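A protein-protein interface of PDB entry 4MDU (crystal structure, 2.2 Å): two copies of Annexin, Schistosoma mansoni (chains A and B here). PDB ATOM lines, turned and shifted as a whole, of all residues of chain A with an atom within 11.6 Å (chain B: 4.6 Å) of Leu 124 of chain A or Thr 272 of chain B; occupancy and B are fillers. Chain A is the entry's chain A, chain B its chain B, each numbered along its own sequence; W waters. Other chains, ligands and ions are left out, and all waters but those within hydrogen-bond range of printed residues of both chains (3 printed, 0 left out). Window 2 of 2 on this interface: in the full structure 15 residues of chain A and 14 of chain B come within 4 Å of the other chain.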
ATOM      1  N   SER A 116      -3.427  17.605  -8.321  1.00  0.00           N
ATOM      2  CA  SER A 116      -4.165  18.176  -9.456  1.00  0.00           C
ATOM      3  C   SER A 116      -3.552  19.506  -9.923  1.00  0.00           C
ATOM      4  O   SER A 116      -3.403  19.748 -11.117  1.00  0.00           O
ATOM      5  CB  SER A 116      -5.648  18.362  -9.110  1.00  0.00           C
ATOM      6  OG  SER A 116      -6.244  17.121  -8.763  1.00  0.00           O
ATOM      7  N   LEU A 117      -3.192  20.363  -8.979  1.00  0.00           N
ATOM      8  CA  LEU A 117      -2.551  21.628  -9.313  1.00  0.00           C
ATOM      9  C   LEU A 117      -1.215  21.347 -10.005  1.00  0.00           C
ATOM     10  O   LEU A 117      -0.819  22.042 -10.944  1.00  0.00           O
ATOM     11  CB  LEU A 117      -2.324  22.468  -8.045  1.00  0.00           C
ATOM     12  CG  LEU A 117      -3.540  23.059  -7.309  1.00  0.00           C
ATOM     13  CD1 LEU A 117      -3.115  23.696  -5.992  1.00  0.00           C
ATOM     14  CD2 LEU A 117      -4.272  24.070  -8.180  1.00  0.00           C
ATOM     15  N   TYR A 118      -0.515  20.323  -9.531  1.00  0.00           N
ATOM     16  CA  TYR A 118       0.735  19.929 -10.158  1.00  0.00           C
ATOM     17  C   TYR A 118       0.527  19.544 -11.626  1.00  0.00           C
ATOM     18  O   TYR A 118       1.279  19.965 -12.498  1.00  0.00           O
ATOM     19  CB  TYR A 118       1.366  18.759  -9.401  1.00  0.00           C
ATOM     20  CG  TYR A 118       2.573  18.171 -10.107  1.00  0.00           C
ATOM     21  CD1 TYR A 118       2.461  17.022 -10.881  1.00  0.00           C
ATOM     22  CD2 TYR A 118       3.819  18.762  -9.995  1.00  0.00           C
ATOM     23  CE1 TYR A 118       3.555  16.480 -11.519  1.00  0.00           C
ATOM     24  CE2 TYR A 118       4.921  18.228 -10.633  1.00  0.00           C
ATOM     25  CZ  TYR A 118       4.784  17.090 -11.397  1.00  0.00           C
ATOM     26  OH  TYR A 118       5.883  16.562 -12.036  1.00  0.00           O
ATOM     27  N   TYR A 119      -0.485  18.726 -11.895  1.00  0.00           N
ATOM     28  CA  TYR A 119      -0.731  18.279 -13.255  1.00  0.00           C
ATOM     29  C   TYR A 119      -1.281  19.418 -14.112  1.00  0.00           C
ATOM     30  O   TYR A 119      -1.046  19.471 -15.311  1.00  0.00           O
ATOM     31  CB  TYR A 119      -1.660  17.060 -13.282  1.00  0.00           C
ATOM     32  CG  TYR A 119      -0.961  15.784 -12.871  1.00  0.00           C
ATOM     33  CD1 TYR A 119       0.063  15.254 -13.644  1.00  0.00           C
ATOM     34  CD2 TYR A 119      -1.317  15.112 -11.711  1.00  0.00           C
ATOM     35  CE1 TYR A 119       0.717  14.092 -13.271  1.00  0.00           C
ATOM     36  CE2 TYR A 119      -0.675  13.946 -11.330  1.00  0.00           C
ATOM     37  CZ  TYR A 119       0.338  13.441 -12.116  1.00  0.00           C
ATOM     38  OH  TYR A 119       0.978  12.281 -11.743  1.00  0.00           O
ATOM     39  N   ALA A 120      -2.001  20.342 -13.490  1.00  0.00           N
ATOM     40  CA  ALA A 120      -2.555  21.456 -14.236  1.00  0.00           C
ATOM     41  C   ALA A 120      -1.439  22.377 -14.705  1.00  0.00           C
ATOM     42  O   ALA A 120      -1.576  23.039 -15.724  1.00  0.00           O
ATOM     43  CB  ALA A 120      -3.561  22.232 -13.395  1.00  0.00           C
ATOM     44  N   MET A 121      -0.337  22.425 -13.969  1.00  0.00           N
ATOM     45  CA  MET A 121       0.734  23.366 -14.322  1.00  0.00           C
ATOM     46  C   MET A 121       1.906  22.756 -15.090  1.00  0.00           C
ATOM     47  O   MET A 121       2.555  23.438 -15.875  1.00  0.00           O
ATOM     48  CB  MET A 121       1.242  24.105 -13.085  1.00  0.00           C
ATOM     49  CG  MET A 121       0.238  25.078 -12.497  1.00  0.00           C
ATOM     50  SD  MET A 121       0.928  25.983 -11.105  1.00  0.00           S
ATOM     51  CE  MET A 121       0.957  24.729  -9.833  1.00  0.00           C
ATOM     52  N   LYS A 122       2.172  21.475 -14.878  1.00  0.00           N
ATOM     53  CA  LYS A 122       3.366  20.858 -15.456  1.00  0.00           C
ATOM     54  C   LYS A 122       3.198  20.309 -16.870  1.00  0.00           C
ATOM     55  O   LYS A 122       4.187  20.062 -17.553  1.00  0.00           O
ATOM     56  CB  LYS A 122       3.916  19.773 -14.531  1.00  0.00           C
ATOM     57  N   GLY A 123       1.959  20.112 -17.306  1.00  0.00           N
ATOM     58  CA  GLY A 123       1.719  19.665 -18.666  1.00  0.00           C
ATOM     59  C   GLY A 123       2.074  20.736 -19.684  1.00  0.00           C
ATOM     60  O   GLY A 123       2.622  21.780 -19.340  1.00  0.00           O
ATOM     61  N   LEU A 124       1.777  20.469 -20.947  1.00  0.00           N
ATOM     62  CA  LEU A 124       1.911  21.477 -21.988  1.00  0.00           C
ATOM     63  C   LEU A 124       0.715  22.408 -21.921  1.00  0.00           C
ATOM     64  O   LEU A 124      -0.426  21.970 -22.018  1.00  0.00           O
ATOM     65  CB  LEU A 124       1.978  20.820 -23.368  1.00  0.00           C
ATOM     66  CG  LEU A 124       3.332  20.215 -23.736  1.00  0.00           C
ATOM     67  CD1 LEU A 124       3.286  19.592 -25.121  1.00  0.00           C
ATOM     68  CD2 LEU A 124       4.405  21.295 -23.658  1.00  0.00           C
ATOM     69  N   GLY A 125       0.973  23.693 -21.769  1.00  0.00           N
ATOM     70  CA  GLY A 125      -0.111  24.625 -21.547  1.00  0.00           C
ATOM     71  C   GLY A 125      -0.585  24.511 -20.108  1.00  0.00           C
ATOM     72  O   GLY A 125      -0.437  23.473 -19.470  1.00  0.00           O
ATOM     73  N   THR A 126      -1.157  25.588 -19.602  1.00  0.00           N
ATOM     74  CA  THR A 126      -1.640  25.648 -18.236  1.00  0.00           C
ATOM     75  C   THR A 126      -3.142  25.372 -18.181  1.00  0.00           C
ATOM     76  O   THR A 126      -3.932  26.032 -18.843  1.00  0.00           O
ATOM     77  CB  THR A 126      -1.357  27.033 -17.656  1.00  0.00           C
ATOM     78  OG1 THR A 126       0.049  27.261 -17.718  1.00  0.00           O
ATOM     79  CG2 THR A 126      -1.817  27.121 -16.207  1.00  0.00           C
ATOM     80  N   ASN A 127      -3.537  24.379 -17.400  1.00  0.00           N
ATOM     81  CA  ASN A 127      -4.951  24.116 -17.221  1.00  0.00           C
ATOM     82  C   ASN A 127      -5.544  25.060 -16.164  1.00  0.00           C
ATOM     83  O   ASN A 127      -5.778  24.678 -15.020  1.00  0.00           O
ATOM     84  CB  ASN A 127      -5.192  22.656 -16.835  1.00  0.00           C
ATOM     85  CG  ASN A 127      -6.650  22.271 -16.988  1.00  0.00           C
ATOM     86  OD1 ASN A 127      -7.527  23.134 -16.910  1.00  0.00           O
ATOM     87  ND2 ASN A 127      -6.920  20.985 -17.217  1.00  0.00           N
ATOM     88  N   ASP A 128      -5.774  26.303 -16.557  1.00  0.00           N
ATOM     89  CA  ASP A 128      -6.248  27.306 -15.627  1.00  0.00           C
ATOM     90  C   ASP A 128      -7.625  26.977 -15.037  1.00  0.00           C
ATOM     91  O   ASP A 128      -7.908  27.321 -13.887  1.00  0.00           O
ATOM     92  CB  ASP A 128      -6.279  28.664 -16.319  1.00  0.00           C
ATOM     93  CG  ASP A 128      -4.892  29.198 -16.584  1.00  0.00           C
ATOM     94  OD1 ASP A 128      -4.242  29.669 -15.625  1.00  0.00           O
ATOM     95  OD2 ASP A 128      -4.450  29.125 -17.745  1.00  0.00           O
ATOM     96  N   ARG A 129      -8.482  26.315 -15.815  1.00  0.00           N
ATOM     97  CA  ARG A 129      -9.791  25.920 -15.299  1.00  0.00           C
ATOM     98  C   ARG A 129      -9.622  25.219 -13.960  1.00  0.00           C
ATOM     99  O   ARG A 129     -10.341  25.500 -13.010  1.00  0.00           O
ATOM    100  CB  ARG A 129     -10.528  25.002 -16.276  1.00  0.00           C
ATOM    101  CG  ARG A 129     -11.736  24.301 -15.646  1.00  0.00           C
ATOM    102  CD  ARG A 129     -12.425  23.340 -16.619  1.00  0.00           C
ATOM    103  NE  ARG A 129     -11.510  22.360 -17.207  1.00  0.00           N
ATOM    104  CZ  ARG A 129     -11.138  21.225 -16.615  1.00  0.00           C
ATOM    105  NH1 ARG A 129     -11.585  20.922 -15.404  1.00  0.00           N
ATOM    106  NH2 ARG A 129     -10.304  20.396 -17.230  1.00  0.00           N
ATOM    107  N   VAL A 130      -8.660  24.305 -13.891  1.00  0.00           N
ATOM    108  CA  VAL A 130      -8.409  23.569 -12.664  1.00  0.00           C
ATOM    109  C   VAL A 130      -7.830  24.476 -11.568  1.00  0.00           C
ATOM    110  O   VAL A 130      -8.152  24.329 -10.384  1.00  0.00           O
ATOM    111  CB  VAL A 130      -7.452  22.380 -12.924  1.00  0.00           C
ATOM    112  CG1 VAL A 130      -7.000  21.750 -11.602  1.00  0.00           C
ATOM    113  CG2 VAL A 130      -8.125  21.351 -13.820  1.00  0.00           C
ATOM    114  N   LEU A 131      -6.956  25.404 -11.944  1.00  0.00           N
ATOM    115  CA  LEU A 131      -6.424  26.333 -10.952  1.00  0.00           C
ATOM    116  C   LEU A 131      -7.586  27.131 -10.345  1.00  0.00           C
ATOM    117  O   LEU A 131      -7.692  27.312  -9.123  1.00  0.00           O
ATOM    118  CB  LEU A 131      -5.376  27.278 -11.568  1.00  0.00           C
ATOM    119  CG  LEU A 131      -4.102  26.660 -12.179  1.00  0.00           C
ATOM    120  CD1 LEU A 131      -3.094  27.733 -12.559  1.00  0.00           C
ATOM    121  CD2 LEU A 131      -3.450  25.641 -11.245  1.00  0.00           C
ATOM    122  N   ARG A 164      11.814  24.538  -4.790  1.00  0.00           N
ATOM    123  CA  ARG A 164      10.697  24.624  -5.721  1.00  0.00           C
ATOM    124  C   ARG A 164       9.420  24.645  -4.886  1.00  0.00           C
ATOM    125  O   ARG A 164       9.332  23.974  -3.862  1.00  0.00           O
ATOM    126  CB  ARG A 164      10.693  23.425  -6.679  1.00  0.00           C
ATOM    127  CG  ARG A 164       9.876  23.611  -7.957  1.00  0.00           C
ATOM    128  CD  ARG A 164       9.956  22.380  -8.857  1.00  0.00           C
ATOM    129  NE  ARG A 164       8.927  22.400  -9.897  1.00  0.00           N
ATOM    130  CZ  ARG A 164       8.679  21.392 -10.733  1.00  0.00           C
ATOM    131  NH1 ARG A 164       9.396  20.275 -10.671  1.00  0.00           N
ATOM    132  NH2 ARG A 164       7.716  21.500 -11.640  1.00  0.00           N
ATOM    133  N   LYS A 171       2.719  31.138 -12.571  1.00  0.00           N
ATOM    134  CA  LYS A 171       3.074  32.287 -13.385  1.00  0.00           C
ATOM    135  C   LYS A 171       3.325  33.517 -12.508  1.00  0.00           C
ATOM    136  O   LYS A 171       2.770  33.628 -11.414  1.00  0.00           O
ATOM    137  CB  LYS A 171       1.968  32.559 -14.406  1.00  0.00           C
ATOM    138  CG  LYS A 171       1.631  31.345 -15.268  1.00  0.00           C
ATOM    139  CD  LYS A 171       0.770  31.731 -16.463  1.00  0.00           C
ATOM    140  CE  LYS A 171      -0.111  30.571 -16.927  1.00  0.00           C
ATOM    141  NZ  LYS A 171      -1.531  30.706 -16.447  1.00  0.00           N
ATOM    142  N   LEU A 305     -15.153  11.803 -20.788  1.00  0.00           N
ATOM    143  CA  LEU A 305     -13.702  11.645 -20.724  1.00  0.00           C
ATOM    144  C   LEU A 305     -13.288  10.572 -19.719  1.00  0.00           C
ATOM    145  O   LEU A 305     -12.161  10.089 -19.752  1.00  0.00           O
ATOM    146  CB  LEU A 305     -13.015  12.975 -20.380  1.00  0.00           C
ATOM    147  CG  LEU A 305     -12.970  14.069 -21.452  1.00  0.00           C
ATOM    148  CD1 LEU A 305     -12.417  15.373 -20.879  1.00  0.00           C
ATOM    149  CD2 LEU A 305     -12.154  13.611 -22.655  1.00  0.00           C
ATOM    150  N   LYS A 308      -9.864  10.355 -17.859  1.00  0.00           N
ATOM    151  CA  LYS A 308      -8.993  11.231 -18.639  1.00  0.00           C
ATOM    152  C   LYS A 308      -9.023  12.661 -18.087  1.00  0.00           C
ATOM    153  O   LYS A 308      -8.032  13.389 -18.171  1.00  0.00           O
ATOM    154  CB  LYS A 308      -9.349  11.199 -20.133  1.00  0.00           C
ATOM    155  CG  LYS A 308      -8.657  10.080 -20.907  1.00  0.00           C
ATOM    156  CD  LYS A 308      -8.914  10.170 -22.407  1.00  0.00           C
ATOM    157  CE  LYS A 308     -10.106   9.322 -22.815  1.00  0.00           C
ATOM    158  N   ASP A 309     -10.159  13.056 -17.518  1.00  0.00           N
ATOM    159  CA  ASP A 309     -10.245  14.327 -16.810  1.00  0.00           C
ATOM    160  C   ASP A 309     -10.676  14.105 -15.364  1.00  0.00           C
ATOM    161  O   ASP A 309     -11.616  13.359 -15.106  1.00  0.00           O
ATOM    162  CB  ASP A 309     -11.217  15.268 -17.504  1.00  0.00           C
ATOM    163  CG  ASP A 309     -11.335  16.587 -16.790  1.00  0.00           C
ATOM    164  OD1 ASP A 309     -10.422  17.420 -16.957  1.00  0.00           O
ATOM    165  OD2 ASP A 309     -12.329  16.786 -16.056  1.00  0.00           O
ATOM    166  N   ASP B 177       3.377  28.414 -22.074  1.00  0.00           N
ATOM    167  CA  ASP B 177       3.345  27.880 -23.426  1.00  0.00           C
ATOM    168  C   ASP B 177       2.384  28.655 -24.323  1.00  0.00           C
ATOM    169  O   ASP B 177       2.660  28.869 -25.506  1.00  0.00           O
ATOM    170  CB  ASP B 177       3.001  26.388 -23.407  1.00  0.00           C
ATOM    171  CG  ASP B 177       3.984  25.575 -22.567  1.00  0.00           C
ATOM    172  OD1 ASP B 177       5.198  25.827 -22.673  1.00  0.00           O
ATOM    173  OD2 ASP B 177       3.550  24.691 -21.797  1.00  0.00           O
ATOM    174  N   ILE B 237       5.776  21.414 -30.880  1.00  0.00           N
ATOM    175  CA  ILE B 237       4.393  21.497 -31.314  1.00  0.00           C
ATOM    176  C   ILE B 237       4.133  22.910 -31.811  1.00  0.00           C
ATOM    177  O   ILE B 237       3.540  23.105 -32.869  1.00  0.00           O
ATOM    178  CB  ILE B 237       3.421  21.124 -30.186  1.00  0.00           C
ATOM    179  CG1 ILE B 237       3.785  19.744 -29.636  1.00  0.00           C
ATOM    180  CG2 ILE B 237       1.977  21.152 -30.683  1.00  0.00           C
ATOM    181  CD1 ILE B 237       2.795  19.189 -28.661  1.00  0.00           C
ATOM    182  N   ILE B 268      -3.135  16.730 -30.247  1.00  0.00           N
ATOM    183  CA  ILE B 268      -3.025  18.044 -29.622  1.00  0.00           C
ATOM    184  C   ILE B 268      -3.994  18.168 -28.455  1.00  0.00           C
ATOM    185  O   ILE B 268      -3.632  18.636 -27.380  1.00  0.00           O
ATOM    186  CB  ILE B 268      -3.258  19.165 -30.643  1.00  0.00           C
ATOM    187  CG1 ILE B 268      -1.998  19.310 -31.518  1.00  0.00           C
ATOM    188  CG2 ILE B 268      -3.635  20.464 -29.933  1.00  0.00           C
ATOM    189  CD1 ILE B 268      -2.097  20.326 -32.610  1.00  0.00           C
ATOM    190  N   GLU B 269      -5.220  17.710 -28.663  1.00  0.00           N
ATOM    191  CA  GLU B 269      -6.261  17.853 -27.652  1.00  0.00           C
ATOM    192  C   GLU B 269      -5.986  17.066 -26.372  1.00  0.00           C
ATOM    193  O   GLU B 269      -6.430  17.451 -25.290  1.00  0.00           O
ATOM    194  CB  GLU B 269      -7.621  17.495 -28.243  1.00  0.00           C
ATOM    195  CG  GLU B 269      -8.142  18.570 -29.177  1.00  0.00           C
ATOM    196  CD  GLU B 269      -9.463  18.207 -29.813  1.00  0.00           C
ATOM    197  OE1 GLU B 269      -9.698  17.002 -30.065  1.00  0.00           O
ATOM    198  OE2 GLU B 269     -10.262  19.134 -30.066  1.00  0.00           O
ATOM    199  N   SER B 270      -5.232  15.979 -26.480  1.00  0.00           N
ATOM    200  CA  SER B 270      -4.938  15.175 -25.304  1.00  0.00           C
ATOM    201  C   SER B 270      -3.615  15.547 -24.635  1.00  0.00           C
ATOM    202  O   SER B 270      -3.381  15.191 -23.488  1.00  0.00           O
ATOM    203  CB  SER B 270      -4.972  13.680 -25.643  1.00  0.00           C
ATOM    204  OG  SER B 270      -4.039  13.357 -26.657  1.00  0.00           O
ATOM    205  N   GLU B 271      -2.751  16.265 -25.339  1.00  0.00           N
ATOM    206  CA  GLU B 271      -1.419  16.541 -24.808  1.00  0.00           C
ATOM    207  C   GLU B 271      -1.279  17.934 -24.230  1.00  0.00           C
ATOM    208  O   GLU B 271      -0.350  18.203 -23.470  1.00  0.00           O
ATOM    209  CB  GLU B 271      -0.353  16.342 -25.882  1.00  0.00           C
ATOM    210  CG  GLU B 271      -0.205  14.910 -26.330  1.00  0.00           C
ATOM    211  CD  GLU B 271       0.045  13.981 -25.168  1.00  0.00           C
ATOM    212  OE1 GLU B 271      -0.885  13.233 -24.808  1.00  0.00           O
ATOM    213  OE2 GLU B 271       1.167  14.007 -24.612  1.00  0.00           O
ATOM    214  N   THR B 272      -2.193  18.821 -24.599  1.00  0.00           N
ATOM    215  CA  THR B 272      -2.087  20.214 -24.193  1.00  0.00           C
ATOM    216  C   THR B 272      -3.345  20.639 -23.469  1.00  0.00           C
ATOM    217  O   THR B 272      -4.375  19.974 -23.565  1.00  0.00           O
ATOM    218  CB  THR B 272      -1.888  21.129 -25.403  1.00  0.00           C
ATOM    219  OG1 THR B 272      -3.054  21.077 -26.239  1.00  0.00           O
ATOM    220  CG2 THR B 272      -0.672  20.685 -26.201  1.00  0.00           C
ATOM    221  N   SER B 273      -3.263  21.754 -22.752  1.00  0.00           N
ATOM    222  CA  SER B 273      -4.383  22.225 -21.953  1.00  0.00           C
ATOM    223  C   SER B 273      -4.497  23.721 -22.033  1.00  0.00           C
ATOM    224  O   SER B 273      -3.580  24.393 -22.519  1.00  0.00           O
ATOM    225  CB  SER B 273      -4.172  21.841 -20.492  1.00  0.00           C
ATOM    226  OG  SER B 273      -3.889  20.467 -20.401  1.00  0.00           O
ATOM    227  N   TYR B 276      -3.478  27.377 -24.374  1.00  0.00           N
ATOM    228  CA  TYR B 276      -2.480  26.802 -25.260  1.00  0.00           C
ATOM    229  C   TYR B 276      -3.134  25.781 -26.189  1.00  0.00           C
ATOM    230  O   TYR B 276      -2.941  25.817 -27.410  1.00  0.00           O
ATOM    231  CB  TYR B 276      -1.319  26.192 -24.469  1.00  0.00           C
ATOM    232  CG  TYR B 276      -0.218  25.639 -25.347  1.00  0.00           C
ATOM    233  CD1 TYR B 276       0.485  26.468 -26.214  1.00  0.00           C
ATOM    234  CD2 TYR B 276       0.127  24.295 -25.297  1.00  0.00           C
ATOM    235  CE1 TYR B 276       1.484  25.976 -27.008  1.00  0.00           C
ATOM    236  CE2 TYR B 276       1.129  23.789 -26.091  1.00  0.00           C
ATOM    237  CZ  TYR B 276       1.803  24.633 -26.944  1.00  0.00           C
ATOM    238  OH  TYR B 276       2.796  24.136 -27.738  1.00  0.00           O
ATOM    239  N   ARG B 277      -3.946  24.892 -25.622  1.00  0.00           N
ATOM    240  CA  ARG B 277      -4.695  23.947 -26.456  1.00  0.00           C
ATOM    241  C   ARG B 277      -5.618  24.673 -27.426  1.00  0.00           C
ATOM    242  O   ARG B 277      -5.674  24.348 -28.615  1.00  0.00           O
ATOM    243  CB  ARG B 277      -5.476  22.957 -25.586  1.00  0.00           C
ATOM    244  CG  ARG B 277      -6.618  22.257 -26.307  1.00  0.00           C
ATOM    245  CD  ARG B 277      -7.183  21.128 -25.469  1.00  0.00           C
ATOM    246  NE  ARG B 277      -7.329  21.528 -24.075  1.00  0.00           N
ATOM    247  CZ  ARG B 277      -7.633  20.694 -23.083  1.00  0.00           C
ATOM    248  NH1 ARG B 277      -7.828  19.400 -23.331  1.00  0.00           N
ATOM    249  NH2 ARG B 277      -7.738  21.152 -21.840  1.00  0.00           N
ATOM    250  N   LEU B 280      -3.630  26.289 -30.290  1.00  0.00           N
ATOM    251  CA  LEU B 280      -3.194  25.234 -31.215  1.00  0.00           C
ATOM    252  C   LEU B 280      -4.376  24.658 -31.989  1.00  0.00           C
ATOM    253  O   LEU B 280      -4.296  24.457 -33.203  1.00  0.00           O
ATOM    254  CB  LEU B 280      -2.487  24.107 -30.460  1.00  0.00           C
ATOM    255  CG  LEU B 280      -1.176  24.471 -29.752  1.00  0.00           C
ATOM    256  CD1 LEU B 280      -0.591  23.278 -29.006  1.00  0.00           C
ATOM    257  CD2 LEU B 280      -0.199  24.970 -30.772  1.00  0.00           C
HETATM  258  O   HOH W   1      -2.584  27.513 -21.486  1.00  0.00           O
HETATM  259  O   HOH W   2       0.228  28.266 -21.086  1.00  0.00           O
HETATM  260  O   HOH W   3       2.674  26.958 -19.667  1.00  0.00           O
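Leu 124 of chain A touches six residues of chain B. Of the printed residues of chain B, Gly 125 of chain A touches Asp 177, Ser 273 and Tyr 276. Printed residues of chain B within 4 Å of Thr 126 of chain A: Ser 273. Of the printed residues of chain B, Asn 127 of chain A touches Ser 273. Arg 164 of chain A touches none of the printed residues of chain B. Lys 171 of chain A touches none of the printed residues of chain B. Of the printed residues of chain A, Asp 177 of chain B touches Gly 123 (3.9 Å), Leu 124 (3.6 Å) and Gly 125 (2.8 Å). Printed residues of chain A within 4 Å of Ile 237 of chain B: Leu 124. No residue of chain A comes within 4 Å of Ile 268 of chain B. No residue of chain A comes within 4 Å of Ser 270 of chain B. Of chain A, only Leu 124 (3.5 Å) comes within 4 Å of Glu 271 of chain B. Printed residues of chain A within 4 Å of Thr 272 of chain B: Leu 124. Arg 277 of chain B touches none of the printed residues of chain A. The nearest printed residue of chain B that does not touch Leu 124 of chain A is Arg 277 of chain B (5.8 Å).
Of the 11 printed residues of chain B, 6 touch a printed residue of chain A. Along chain B the printed residues that touch a printed residue of chain A span positions 177 to 276. Of the 21 printed residues of chain A, 5 touch a printed residue of chain B. Along chain A the printed residues that touch a printed residue of chain B span positions 123 to 127. Among the printed residues, 12 pairs touch across the chains.
The backbone NH of Gly 125 of chain A sits at hydrogen-bond distance from the side-chain carboxylate of Asp 177 of chain B (2.8 Å). O of Leu 124 of chain A is in hydrogen-bond range of N of Ser 273 of chain B, 2.9 Å away.
No position is printed for both chains.
Water W3 bridges N of Asp 177 of chain B and OG1 of Thr 126 of chain A. Water W1 lies within hydrogen-bond range of N of Tyr 276 of chain B (3.0 Å), N of Thr 126 of chain A (3.0 Å) and O of Ser 273 of chain B (3.4 Å). Water W2 lies within hydrogen-bond range of the backbone NH of Asp 177 of chain B (3.3 Å) and the backbone NH of Thr 126 of chain A (3.4 Å).
O of Thr 272 of chain B sits close to NE of Arg 277 of chain B. O of Ile 268 of chain B is in hydrogen-bond range of OG1 of Thr 272 of chain B. NH2 of Arg 129 of chain A sits close to ND2 of Asn 127 of chain A. N of Asn 127 of chain A sits at hydrogen-bond distance from O of Ala 120 of chain A, at 2.9 Å. N of Val 130 of chain A is in hydrogen-bond range of OD1 of Asn 127 of chain A (3.4 Å).
O of Gly 123 of chain A touches OD2 of Asp 177 of chain B, 3.9 Å away. CA of Leu 124 of chain A touches OD2 of Asp 177 of chain B (3.6 Å). CD1 of Ile 237 of chain B touches CD1 of Leu 124 of chain A, 3.6 Å away. Leu 124 of chain A touches Glu 271 of chain B. Leu 124 of chain A touches Thr 272 of chain B (O to CA, 3.3 Å). Leu 124 of chain A touches Tyr 276 of chain B (C to CD2, 3.9 Å). Ser 273 of chain B touches Gly 125 of chain A (O to CA, 3.6 Å). Gly 125 of chain A touches Tyr 276 of chain B. Ser 273 of chain B touches Thr 126 of chain A (O to N, 3.98 Å). Asn 127 of chain A touches Ser 273 of chain B (CB to CB, 3.9 Å).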
